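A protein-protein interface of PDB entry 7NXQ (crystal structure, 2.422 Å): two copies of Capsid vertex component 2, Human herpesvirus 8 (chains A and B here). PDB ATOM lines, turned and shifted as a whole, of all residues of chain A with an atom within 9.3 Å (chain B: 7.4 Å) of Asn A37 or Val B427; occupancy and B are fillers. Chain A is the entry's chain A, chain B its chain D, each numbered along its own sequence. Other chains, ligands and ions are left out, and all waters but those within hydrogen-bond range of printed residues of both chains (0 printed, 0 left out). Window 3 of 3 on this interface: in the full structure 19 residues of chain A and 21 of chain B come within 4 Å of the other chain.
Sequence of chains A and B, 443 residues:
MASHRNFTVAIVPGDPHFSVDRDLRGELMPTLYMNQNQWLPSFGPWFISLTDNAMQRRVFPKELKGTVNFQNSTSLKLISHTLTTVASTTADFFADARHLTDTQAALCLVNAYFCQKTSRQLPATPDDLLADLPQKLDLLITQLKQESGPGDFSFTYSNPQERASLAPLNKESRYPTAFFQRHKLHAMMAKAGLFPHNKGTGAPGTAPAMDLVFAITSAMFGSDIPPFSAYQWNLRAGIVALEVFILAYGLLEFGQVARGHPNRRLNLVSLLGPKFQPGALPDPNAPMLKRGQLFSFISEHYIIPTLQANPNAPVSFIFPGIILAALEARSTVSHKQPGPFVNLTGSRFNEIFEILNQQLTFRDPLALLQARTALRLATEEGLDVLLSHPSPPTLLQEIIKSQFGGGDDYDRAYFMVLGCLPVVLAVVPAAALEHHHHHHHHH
The side-chain amide nitrogen of Gln A38 lies within hydrogen-bond range of the backbone carbonyl oxygen of Ala B426, 3.4 Å away. The backbone NH of Asn B72 is in hydrogen-bond range of the backbone carbonyl oxygen of Met A34. OE1 of Gln B71 sits at hydrogen-bond distance from ND2 of Asn A37 (3.3 Å). O of Phe B70 sits at hydrogen-bond distance from N of Gln A36, at 3.0 Å.
Of the 15 printed residues of chain A, 6 touch a printed residue of chain B. Hydrophobic or aromatic side chains of chain A that line the printed part of chain B: Met A34. Along chain A the printed residues that touch a printed residue of chain B span positions 33 to 38. Printed residues of chain B that touch a printed residue of chain A: Phe B70, Gln B71, Asn B72, Ala B426, Val B427 and Pro B429. Hydrophobic or aromatic side chains of chain B within 4 Å of the printed part of chain A: Phe B70, Val B427 and Pro B429. Among the printed residues, no Asp or Glu carboxylate lies within 4 Å of a Lys or Arg side-chain nitrogen of the other chain.
Asn A37 touches Gln B71, but with the chains exchanged Gln A71 does not touch Asn B37 (16.2 Å). Asn A37 touches Val B427, but with the chains exchanged Val A427 does not touch Asn B37 (12.9 Å). Gln A38 touches Ala B426, but with the chains exchanged Ala A426 does not touch Gln B38 (16.3 Å). Gln A38 touches Pro B429, but with the chains exchanged Pro A429 does not touch Gln B38 (16.7 Å). Positions printed for both chains: 35, 36, 37, 38, 39, 40, 71, 425, 426, 427, 428 and 429. Of the 12 pairs that touch across the chains among the printed residues, none has its exchanged pair printed and touching as well.
The backbone carbonyl oxygen (O) of Gln A38 sits at hydrogen-bond distance from the backbone NH (N) of Val A427 (2.9 Å). The side-chain amide nitrogen (ND2) of Asn A35 lies close to the indole nitrogen (NE1) of Trp A39 (3.4 Å). The side-chain amide oxygen of Gln A38 lies close to the side-chain amide oxygen of Asn A35. N of Val B427 is in hydrogen-bond range of O of Gln B38 (2.9 Å). NE2 of Gln A36 lies within hydrogen-bond range of O of Tyr A33 (2.9 Å).
Printed residues of chain B within 4 Å of Tyr A33: Phe B70. Of the printed residues of chain B, Gln A36 touches Phe B70. Of chain B, only Gln B71 (3.3 Å) and Val B427 (3.6 Å) come within 4 Å of Asn A37. Ala A426 touches none of the printed residues of chain B. Val A428 touches none of the printed residues of chain B. Of the printed residues of chain A, Asn B72 touches Met A34 (2.9 Å), Asn A35 (3.3 Å) and Gln A38 (3.9 Å). Of chain A, only Gln A38 (3.4 Å) comes within 4 Å of Ala B426. Printed residues of chain A within 4 Å of Val B427: Asn A37. No residue of chain A comes within 4 Å of Val B428. Of the printed residues of chain A, Pro B429 touches Gln A38 (3.8 Å). The nearest printed residue of chain B that does not touch Met A34 is Leu B40 (8.8 Å).
Tyr A33 touches Phe B70. Phe B70 touches Met A34 (O to C, 3.4 Å). O of Met A34 touches N of Gln B71, at 3.7 Å. Asn A35 touches Phe B70. Asn A35 touches Asn B72 (OD1 to CB, 3.3 Å). CG1 of Val B427 touches ND2 of Asn A37, at 3.6 Å. Gln A38 touches Asn B72. Gln A38 touches Pro B429.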
ATOM      1  N   LEU A  32      21.628  32.572  10.115  1.00  0.00           N
ATOM      2  CA  LEU A  32      20.501  33.082  10.887  1.00  0.00           C
ATOM      3  C   LEU A  32      19.636  31.965  11.508  1.00  0.00           C
ATOM      4  O   LEU A  32      18.719  32.260  12.273  1.00  0.00           O
ATOM      5  CB  LEU A  32      19.632  34.012  10.019  1.00  0.00           C
ATOM      6  CG  LEU A  32      20.364  35.085   9.199  1.00  0.00           C
ATOM      7  CD1 LEU A  32      19.403  35.901   8.386  1.00  0.00           C
ATOM      8  CD2 LEU A  32      21.207  35.985  10.085  1.00  0.00           C
ATOM      9  N   TYR A  33      19.930  30.692  11.205  1.00  0.00           N
ATOM     10  CA  TYR A  33      19.174  29.550  11.719  1.00  0.00           C
ATOM     11  C   TYR A  33      20.002  28.716  12.692  1.00  0.00           C
ATOM     12  O   TYR A  33      19.767  27.516  12.822  1.00  0.00           O
ATOM     13  CB  TYR A  33      18.724  28.672  10.540  1.00  0.00           C
ATOM     14  CG  TYR A  33      17.804  29.398   9.585  1.00  0.00           C
ATOM     15  CD1 TYR A  33      18.309  30.201   8.575  1.00  0.00           C
ATOM     16  CD2 TYR A  33      16.430  29.296   9.704  1.00  0.00           C
ATOM     17  CE1 TYR A  33      17.469  30.901   7.720  1.00  0.00           C
ATOM     18  CE2 TYR A  33      15.580  29.977   8.845  1.00  0.00           C
ATOM     19  CZ  TYR A  33      16.104  30.768   7.846  1.00  0.00           C
ATOM     20  OH  TYR A  33      15.271  31.430   6.989  1.00  0.00           O
ATOM     21  N   MET A  34      20.965  29.340  13.378  1.00  0.00           N
ATOM     22  CA  MET A  34      21.878  28.646  14.274  1.00  0.00           C
ATOM     23  C   MET A  34      21.643  28.925  15.759  1.00  0.00           C
ATOM     24  O   MET A  34      22.449  28.513  16.593  1.00  0.00           O
ATOM     25  CB  MET A  34      23.323  28.998  13.894  1.00  0.00           C
ATOM     26  CG  MET A  34      23.621  28.819  12.419  1.00  0.00           C
ATOM     27  SD  MET A  34      23.660  27.070  11.970  1.00  0.00           S
ATOM     28  CE  MET A  34      25.121  26.546  12.807  1.00  0.00           C
ATOM     29  N   ASN A  35      20.535  29.582  16.097  1.00  0.00           N
ATOM     30  CA  ASN A  35      20.182  29.933  17.470  1.00  0.00           C
ATOM     31  C   ASN A  35      18.665  29.703  17.638  1.00  0.00           C
ATOM     32  O   ASN A  35      17.969  30.554  18.177  1.00  0.00           O
ATOM     33  CB  ASN A  35      20.505  31.416  17.636  1.00  0.00           C
ATOM     34  CG  ASN A  35      21.034  31.806  18.984  1.00  0.00           C
ATOM     35  OD1 ASN A  35      20.619  31.276  20.051  1.00  0.00           O
ATOM     36  ND2 ASN A  35      21.966  32.763  18.953  1.00  0.00           N
ATOM     37  N   GLN A  36      18.153  28.573  17.130  1.00  0.00           N
ATOM     38  CA  GLN A  36      16.728  28.296  17.023  1.00  0.00           C
ATOM     39  C   GLN A  36      15.971  28.234  18.346  1.00  0.00           C
ATOM     40  O   GLN A  36      14.742  28.349  18.347  1.00  0.00           O
ATOM     41  CB  GLN A  36      16.492  27.047  16.180  1.00  0.00           C
ATOM     42  CG  GLN A  36      16.954  27.284  14.745  1.00  0.00           C
ATOM     43  CD  GLN A  36      16.519  26.223  13.784  1.00  0.00           C
ATOM     44  OE1 GLN A  36      15.531  25.523  14.009  1.00  0.00           O
ATOM     45  NE2 GLN A  36      17.242  26.087  12.683  1.00  0.00           N
ATOM     46  N   ASN A  37      16.686  28.118  19.465  1.00  0.00           N
ATOM     47  CA  ASN A  37      16.058  28.140  20.783  1.00  0.00           C
ATOM     48  C   ASN A  37      15.731  29.575  21.234  1.00  0.00           C
ATOM     49  O   ASN A  37      14.876  29.759  22.100  1.00  0.00           O
ATOM     50  CB  ASN A  37      16.989  27.512  21.823  1.00  0.00           C
ATOM     51  CG  ASN A  37      16.829  26.019  21.955  1.00  0.00           C
ATOM     52  OD1 ASN A  37      15.891  25.409  21.396  1.00  0.00           O
ATOM     53  ND2 ASN A  37      17.742  25.394  22.694  1.00  0.00           N
ATOM     54  N   GLN A  38      16.448  30.583  20.704  1.00  0.00           N
ATOM     55  CA  GLN A  38      16.261  31.962  21.129  1.00  0.00           C
ATOM     56  C   GLN A  38      15.611  32.868  20.101  1.00  0.00           C
ATOM     57  O   GLN A  38      14.816  33.730  20.481  1.00  0.00           O
ATOM     58  CB  GLN A  38      17.590  32.544  21.595  1.00  0.00           C
ATOM     59  CG  GLN A  38      18.046  31.885  22.886  1.00  0.00           C
ATOM     60  CD  GLN A  38      19.544  31.877  23.066  1.00  0.00           C
ATOM     61  OE1 GLN A  38      20.306  32.529  22.316  1.00  0.00           O
ATOM     62  NE2 GLN A  38      19.997  31.111  24.074  1.00  0.00           N
ATOM     63  N   TRP A  39      15.949  32.708  18.820  1.00  0.00           N
ATOM     64  CA  TRP A  39      15.376  33.560  17.792  1.00  0.00           C
ATOM     65  C   TRP A  39      15.381  32.931  16.409  1.00  0.00           C
ATOM     66  O   TRP A  39      16.138  32.000  16.145  1.00  0.00           O
ATOM     67  CB  TRP A  39      16.046  34.948  17.783  1.00  0.00           C
ATOM     68  CG  TRP A  39      17.498  34.953  17.446  1.00  0.00           C
ATOM     69  CD1 TRP A  39      18.545  34.932  18.323  1.00  0.00           C
ATOM     70  CD2 TRP A  39      18.070  35.063  16.133  1.00  0.00           C
ATOM     71  NE1 TRP A  39      19.738  35.012  17.635  1.00  0.00           N
ATOM     72  CE2 TRP A  39      19.473  35.082  16.287  1.00  0.00           C
ATOM     73  CE3 TRP A  39      17.528  35.146  14.838  1.00  0.00           C
ATOM     74  CZ2 TRP A  39      20.342  35.193  15.200  1.00  0.00           C
ATOM     75  CZ3 TRP A  39      18.388  35.283  13.760  1.00  0.00           C
ATOM     76  CH2 TRP A  39      19.778  35.293  13.943  1.00  0.00           C
ATOM     77  N   LEU A  40      14.508  33.442  15.531  1.00  0.00           N
ATOM     78  CA  LEU A  40      14.373  33.001  14.149  1.00  0.00           C
ATOM     79  C   LEU A  40      14.254  34.238  13.258  1.00  0.00           C
ATOM     80  O   LEU A  40      13.688  35.255  13.678  1.00  0.00           O
ATOM     81  CB  LEU A  40      13.141  32.095  13.985  1.00  0.00           C
ATOM     82  CG  LEU A  40      13.282  30.681  14.524  1.00  0.00           C
ATOM     83  CD1 LEU A  40      11.967  29.941  14.469  1.00  0.00           C
ATOM     84  CD2 LEU A  40      14.347  29.921  13.772  1.00  0.00           C
ATOM     85  N   GLN A  71       6.510  29.086  12.324  1.00  0.00           N
ATOM     86  CA  GLN A  71       7.010  29.629  13.577  1.00  0.00           C
ATOM     87  C   GLN A  71       7.411  31.098  13.406  1.00  0.00           C
ATOM     88  O   GLN A  71       8.479  31.491  13.851  1.00  0.00           O
ATOM     89  CB  GLN A  71       8.206  28.789  14.068  1.00  0.00           C
ATOM     90  CG  GLN A  71       7.869  27.335  14.385  1.00  0.00           C
ATOM     91  CD  GLN A  71       9.114  26.573  14.755  1.00  0.00           C
ATOM     92  OE1 GLN A  71       9.978  27.056  15.499  1.00  0.00           O
ATOM     93  NE2 GLN A  71       9.241  25.361  14.241  1.00  0.00           N
ATOM     94  N   LEU A 425      13.750  37.776  15.478  1.00  0.00           N
ATOM     95  CA  LEU A 425      12.561  37.859  16.321  1.00  0.00           C
ATOM     96  C   LEU A 425      12.656  36.775  17.369  1.00  0.00           C
ATOM     97  O   LEU A 425      12.875  35.612  17.027  1.00  0.00           O
ATOM     98  CB  LEU A 425      11.258  37.725  15.526  1.00  0.00           C
ATOM     99  CG  LEU A 425      10.917  38.850  14.549  1.00  0.00           C
ATOM    100  CD1 LEU A 425       9.589  38.585  13.884  1.00  0.00           C
ATOM    101  CD2 LEU A 425      10.908  40.207  15.238  1.00  0.00           C
ATOM    102  N   ALA A 426      12.522  37.153  18.646  1.00  0.00           N
ATOM    103  CA  ALA A 426      12.610  36.207  19.746  1.00  0.00           C
ATOM    104  C   ALA A 426      11.542  35.132  19.646  1.00  0.00           C
ATOM    105  O   ALA A 426      10.390  35.430  19.348  1.00  0.00           O
ATOM    106  CB  ALA A 426      12.502  36.932  21.071  1.00  0.00           C
ATOM    107  N   VAL A 427      11.954  33.876  19.826  1.00  0.00           N
ATOM    108  CA  VAL A 427      11.093  32.699  19.798  1.00  0.00           C
ATOM    109  C   VAL A 427      10.107  32.750  20.986  1.00  0.00           C
ATOM    110  O   VAL A 427       8.926  32.442  20.826  1.00  0.00           O
ATOM    111  CB  VAL A 427      11.971  31.420  19.730  1.00  0.00           C
ATOM    112  CG1 VAL A 427      11.274  30.206  20.332  1.00  0.00           C
ATOM    113  CG2 VAL A 427      12.414  31.147  18.293  1.00  0.00           C
ATOM    114  N   VAL A 428      10.573  33.226  22.150  1.00  0.00           N
ATOM    115  CA  VAL A 428       9.730  33.407  23.325  1.00  0.00           C
ATOM    116  C   VAL A 428       9.396  34.896  23.499  1.00  0.00           C
ATOM    117  O   VAL A 428      10.301  35.726  23.610  1.00  0.00           O
ATOM    118  CB  VAL A 428      10.417  32.854  24.573  1.00  0.00           C
ATOM    119  CG1 VAL A 428       9.592  33.161  25.817  1.00  0.00           C
ATOM    120  CG2 VAL A 428      10.666  31.358  24.431  1.00  0.00           C
ATOM    121  N   PRO A 429       8.104  35.266  23.517  1.00  0.00           N
ATOM    122  CA  PRO A 429       7.754  36.687  23.681  1.00  0.00           C
ATOM    123  C   PRO A 429       7.625  37.056  25.162  1.00  0.00           C
ATOM    124  O   PRO A 429       8.182  38.062  25.603  1.00  0.00           O
ATOM    125  CB  PRO A 429       6.414  36.787  22.954  1.00  0.00           C
ATOM    126  CG  PRO A 429       5.771  35.428  23.202  1.00  0.00           C
ATOM    127  CD  PRO A 429       6.896  34.419  23.415  1.00  0.00           C
ATOM    128  N   ASN B  35      23.112  18.212  30.645  1.00  0.00           N
ATOM    129  CA  ASN B  35      22.117  19.073  31.279  1.00  0.00           C
ATOM    130  C   ASN B  35      21.414  19.851  30.146  1.00  0.00           C
ATOM    131  O   ASN B  35      21.223  21.063  30.247  1.00  0.00           O
ATOM    132  CB  ASN B  35      22.882  20.057  32.167  1.00  0.00           C
ATOM    133  CG  ASN B  35      22.210  20.426  33.449  1.00  0.00           C
ATOM    134  OD1 ASN B  35      20.975  20.558  33.537  1.00  0.00           O
ATOM    135  ND2 ASN B  35      23.033  20.618  34.479  1.00  0.00           N
ATOM    136  N   GLN B  36      21.049  19.152  29.056  1.00  0.00           N
ATOM    137  CA  GLN B  36      20.528  19.747  27.832  1.00  0.00           C
ATOM    138  C   GLN B  36      19.219  20.523  27.989  1.00  0.00           C
ATOM    139  O   GLN B  36      18.890  21.331  27.125  1.00  0.00           O
ATOM    140  CB  GLN B  36      20.434  18.691  26.736  1.00  0.00           C
ATOM    141  CG  GLN B  36      21.830  18.189  26.377  1.00  0.00           C
ATOM    142  CD  GLN B  36      21.855  17.342  25.140  1.00  0.00           C
ATOM    143  OE1 GLN B  36      20.973  17.420  24.279  1.00  0.00           O
ATOM    144  NE2 GLN B  36      22.874  16.518  25.020  1.00  0.00           N
ATOM    145  N   ASN B  37      18.521  20.341  29.095  1.00  0.00           N
ATOM    146  CA  ASN B  37      17.299  21.087  29.385  1.00  0.00           C
ATOM    147  C   ASN B  37      17.615  22.491  29.924  1.00  0.00           C
ATOM    148  O   ASN B  37      16.766  23.380  29.824  1.00  0.00           O
ATOM    149  CB  ASN B  37      16.461  20.346  30.437  1.00  0.00           C
ATOM    150  CG  ASN B  37      15.514  19.325  29.851  1.00  0.00           C
ATOM    151  OD1 ASN B  37      15.297  19.268  28.621  1.00  0.00           O
ATOM    152  ND2 ASN B  37      14.923  18.503  30.725  1.00  0.00           N
ATOM    153  N   GLN B  38      18.796  22.682  30.547  1.00  0.00           N
ATOM    154  CA  GLN B  38      19.148  23.961  31.149  1.00  0.00           C
ATOM    155  C   GLN B  38      20.243  24.740  30.423  1.00  0.00           C
ATOM    156  O   GLN B  38      20.160  25.968  30.365  1.00  0.00           O
ATOM    157  CB  GLN B  38      19.518  23.755  32.610  1.00  0.00           C
ATOM    158  CG  GLN B  38      18.296  23.365  33.418  1.00  0.00           C
ATOM    159  CD  GLN B  38      18.608  22.549  34.648  1.00  0.00           C
ATOM    160  OE1 GLN B  38      19.778  22.394  35.061  1.00  0.00           O
ATOM    161  NE2 GLN B  38      17.556  21.998  35.241  1.00  0.00           N
ATOM    162  N   TRP B  39      21.268  24.056  29.907  1.00  0.00           N
ATOM    163  CA  TRP B  39      22.348  24.743  29.231  1.00  0.00           C
ATOM    164  C   TRP B  39      23.085  23.872  28.227  1.00  0.00           C
ATOM    165  O   TRP B  39      23.014  22.650  28.293  1.00  0.00           O
ATOM    166  CB  TRP B  39      23.312  25.393  30.239  1.00  0.00           C
ATOM    167  CG  TRP B  39      24.039  24.435  31.123  1.00  0.00           C
ATOM    168  CD1 TRP B  39      23.674  24.043  32.378  1.00  0.00           C
ATOM    169  CD2 TRP B  39      25.304  23.811  30.856  1.00  0.00           C
ATOM    170  NE1 TRP B  39      24.627  23.200  32.906  1.00  0.00           N
ATOM    171  CE2 TRP B  39      25.635  23.037  31.986  1.00  0.00           C
ATOM    172  CE3 TRP B  39      26.191  23.827  29.762  1.00  0.00           C
ATOM    173  CZ2 TRP B  39      26.820  22.305  32.065  1.00  0.00           C
ATOM    174  CZ3 TRP B  39      27.365  23.106  29.846  1.00  0.00           C
ATOM    175  CH2 TRP B  39      27.658  22.338  30.979  1.00  0.00           C
ATOM    176  N   LEU B  40      23.781  24.519  27.278  1.00  0.00           N
ATOM    177  CA  LEU B  40      24.583  23.869  26.244  1.00  0.00           C
ATOM    178  C   LEU B  40      25.905  24.618  26.119  1.00  0.00           C
ATOM    179  O   LEU B  40      25.948  25.832  26.317  1.00  0.00           O
ATOM    180  CB  LEU B  40      23.843  23.872  24.893  1.00  0.00           C
ATOM    181  CG  LEU B  40      22.699  22.883  24.760  1.00  0.00           C
ATOM    182  CD1 LEU B  40      21.917  23.131  23.487  1.00  0.00           C
ATOM    183  CD2 LEU B  40      23.199  21.451  24.862  1.00  0.00           C
ATOM    184  N   PRO B  41      27.006  23.923  25.794  1.00  0.00           N
ATOM    185  CA  PRO B  41      28.297  24.615  25.685  1.00  0.00           C
ATOM    186  C   PRO B  41      28.457  25.453  24.422  1.00  0.00           C
ATOM    187  O   PRO B  41      27.821  25.183  23.416  1.00  0.00           O
ATOM    188  CB  PRO B  41      29.307  23.468  25.713  1.00  0.00           C
ATOM    189  CG  PRO B  41      28.579  22.332  25.119  1.00  0.00           C
ATOM    190  CD  PRO B  41      27.147  22.474  25.551  1.00  0.00           C
ATOM    191  N   PHE B  70      22.444  23.713  15.773  1.00  0.00           N
ATOM    192  CA  PHE B  70      21.463  24.760  15.460  1.00  0.00           C
ATOM    193  C   PHE B  70      20.850  25.409  16.709  1.00  0.00           C
ATOM    194  O   PHE B  70      19.860  26.131  16.585  1.00  0.00           O
ATOM    195  CB  PHE B  70      20.343  24.157  14.589  1.00  0.00           C
ATOM    196  CG  PHE B  70      20.873  23.492  13.342  1.00  0.00           C
ATOM    197  CD1 PHE B  70      21.071  24.223  12.181  1.00  0.00           C
ATOM    198  CD2 PHE B  70      21.250  22.156  13.353  1.00  0.00           C
ATOM    199  CE1 PHE B  70      21.608  23.625  11.050  1.00  0.00           C
ATOM    200  CE2 PHE B  70      21.798  21.564  12.223  1.00  0.00           C
ATOM    201  CZ  PHE B  70      21.967  22.301  11.075  1.00  0.00           C
ATOM    202  N   GLN B  71      21.426  25.156  17.902  1.00  0.00           N
ATOM    203  CA  GLN B  71      20.918  25.655  19.172  1.00  0.00           C
ATOM    204  C   GLN B  71      21.996  26.448  19.924  1.00  0.00           C
ATOM    205  O   GLN B  71      22.214  26.217  21.116  1.00  0.00           O
ATOM    206  CB  GLN B  71      20.427  24.465  20.033  1.00  0.00           C
ATOM    207  CG  GLN B  71      19.296  23.674  19.420  1.00  0.00           C
ATOM    208  CD  GLN B  71      18.968  22.487  20.287  1.00  0.00           C
ATOM    209  OE1 GLN B  71      18.883  22.590  21.510  1.00  0.00           O
ATOM    210  NE2 GLN B  71      18.770  21.329  19.681  1.00  0.00           N
ATOM    211  N   ASN B  72      22.670  27.367  19.225  1.00  0.00           N
ATOM    212  CA  ASN B  72      23.738  28.224  19.758  1.00  0.00           C
ATOM    213  C   ASN B  72      24.838  27.399  20.410  1.00  0.00           C
ATOM    214  O   ASN B  72      25.341  27.740  21.478  1.00  0.00           O
ATOM    215  CB  ASN B  72      23.168  29.248  20.736  1.00  0.00           C
ATOM    216  CG  ASN B  72      24.087  30.410  20.998  1.00  0.00           C
ATOM    217  OD1 ASN B  72      24.983  30.714  20.207  1.00  0.00           O
ATOM    218  ND2 ASN B  72      23.879  31.078  22.115  1.00  0.00           N
ATOM    219  N   VAL B 424      29.163  27.916  29.491  1.00  0.00           N
ATOM    220  CA  VAL B 424      27.801  27.394  29.601  1.00  0.00           C
ATOM    221  C   VAL B 424      26.848  28.500  29.207  1.00  0.00           C
ATOM    222  O   VAL B 424      26.985  29.620  29.703  1.00  0.00           O
ATOM    223  CB  VAL B 424      27.458  26.807  30.996  1.00  0.00           C
ATOM    224  CG1 VAL B 424      28.580  25.932  31.513  1.00  0.00           C
ATOM    225  CG2 VAL B 424      27.098  27.886  32.020  1.00  0.00           C
ATOM    226  N   LEU B 425      25.915  28.225  28.286  1.00  0.00           N
ATOM    227  CA  LEU B 425      24.926  29.224  27.903  1.00  0.00           C
ATOM    228  C   LEU B 425      23.543  28.659  28.165  1.00  0.00           C
ATOM    229  O   LEU B 425      23.249  27.553  27.730  1.00  0.00           O
ATOM    230  CB  LEU B 425      25.075  29.654  26.440  1.00  0.00           C
ATOM    231  CG  LEU B 425      26.346  30.434  26.068  1.00  0.00           C
ATOM    232  CD1 LEU B 425      26.327  30.836  24.615  1.00  0.00           C
ATOM    233  CD2 LEU B 425      26.506  31.674  26.918  1.00  0.00           C
ATOM    234  N   ALA B 426      22.709  29.390  28.899  1.00  0.00           N
ATOM    235  CA  ALA B 426      21.358  28.943  29.210  1.00  0.00           C
ATOM    236  C   ALA B 426      20.528  28.708  27.946  1.00  0.00           C
ATOM    237  O   ALA B 426      20.539  29.529  27.021  1.00  0.00           O
ATOM    238  CB  ALA B 426      20.660  29.960  30.101  1.00  0.00           C
ATOM    239  N   VAL B 427      19.846  27.559  27.904  1.00  0.00           N
ATOM    240  CA  VAL B 427      18.967  27.159  26.811  1.00  0.00           C
ATOM    241  C   VAL B 427      17.738  28.100  26.760  1.00  0.00           C
ATOM    242  O   VAL B 427      17.293  28.483  25.680  1.00  0.00           O
ATOM    243  CB  VAL B 427      18.615  25.654  26.953  1.00  0.00           C
ATOM    244  CG1 VAL B 427      17.287  25.303  26.292  1.00  0.00           C
ATOM    245  CG2 VAL B 427      19.735  24.787  26.401  1.00  0.00           C
ATOM    246  N   VAL B 428      17.244  28.525  27.925  1.00  0.00           N
ATOM    247  CA  VAL B 428      16.136  29.462  27.999  1.00  0.00           C
ATOM    248  C   VAL B 428      16.660  30.872  28.332  1.00  0.00           C
ATOM    249  O   VAL B 428      17.330  31.071  29.346  1.00  0.00           O
ATOM    250  CB  VAL B 428      15.082  28.991  29.026  1.00  0.00           C
ATOM    251  CG1 VAL B 428      13.976  30.029  29.190  1.00  0.00           C
ATOM    252  CG2 VAL B 428      14.501  27.642  28.625  1.00  0.00           C
ATOM    253  N   PRO B 429      16.365  31.869  27.481  1.00  0.00           N
ATOM    254  CA  PRO B 429      16.809  33.240  27.778  1.00  0.00           C
ATOM    255  C   PRO B 429      15.757  33.984  28.612  1.00  0.00           C
ATOM    256  O   PRO B 429      16.063  34.592  29.639  1.00  0.00           O
ATOM    257  CB  PRO B 429      16.926  33.859  26.384  1.00  0.00           C
ATOM    258  CG  PRO B 429      15.795  33.192  25.602  1.00  0.00           C
ATOM    259  CD  PRO B 429      15.570  31.817  26.235  1.00  0.00           C
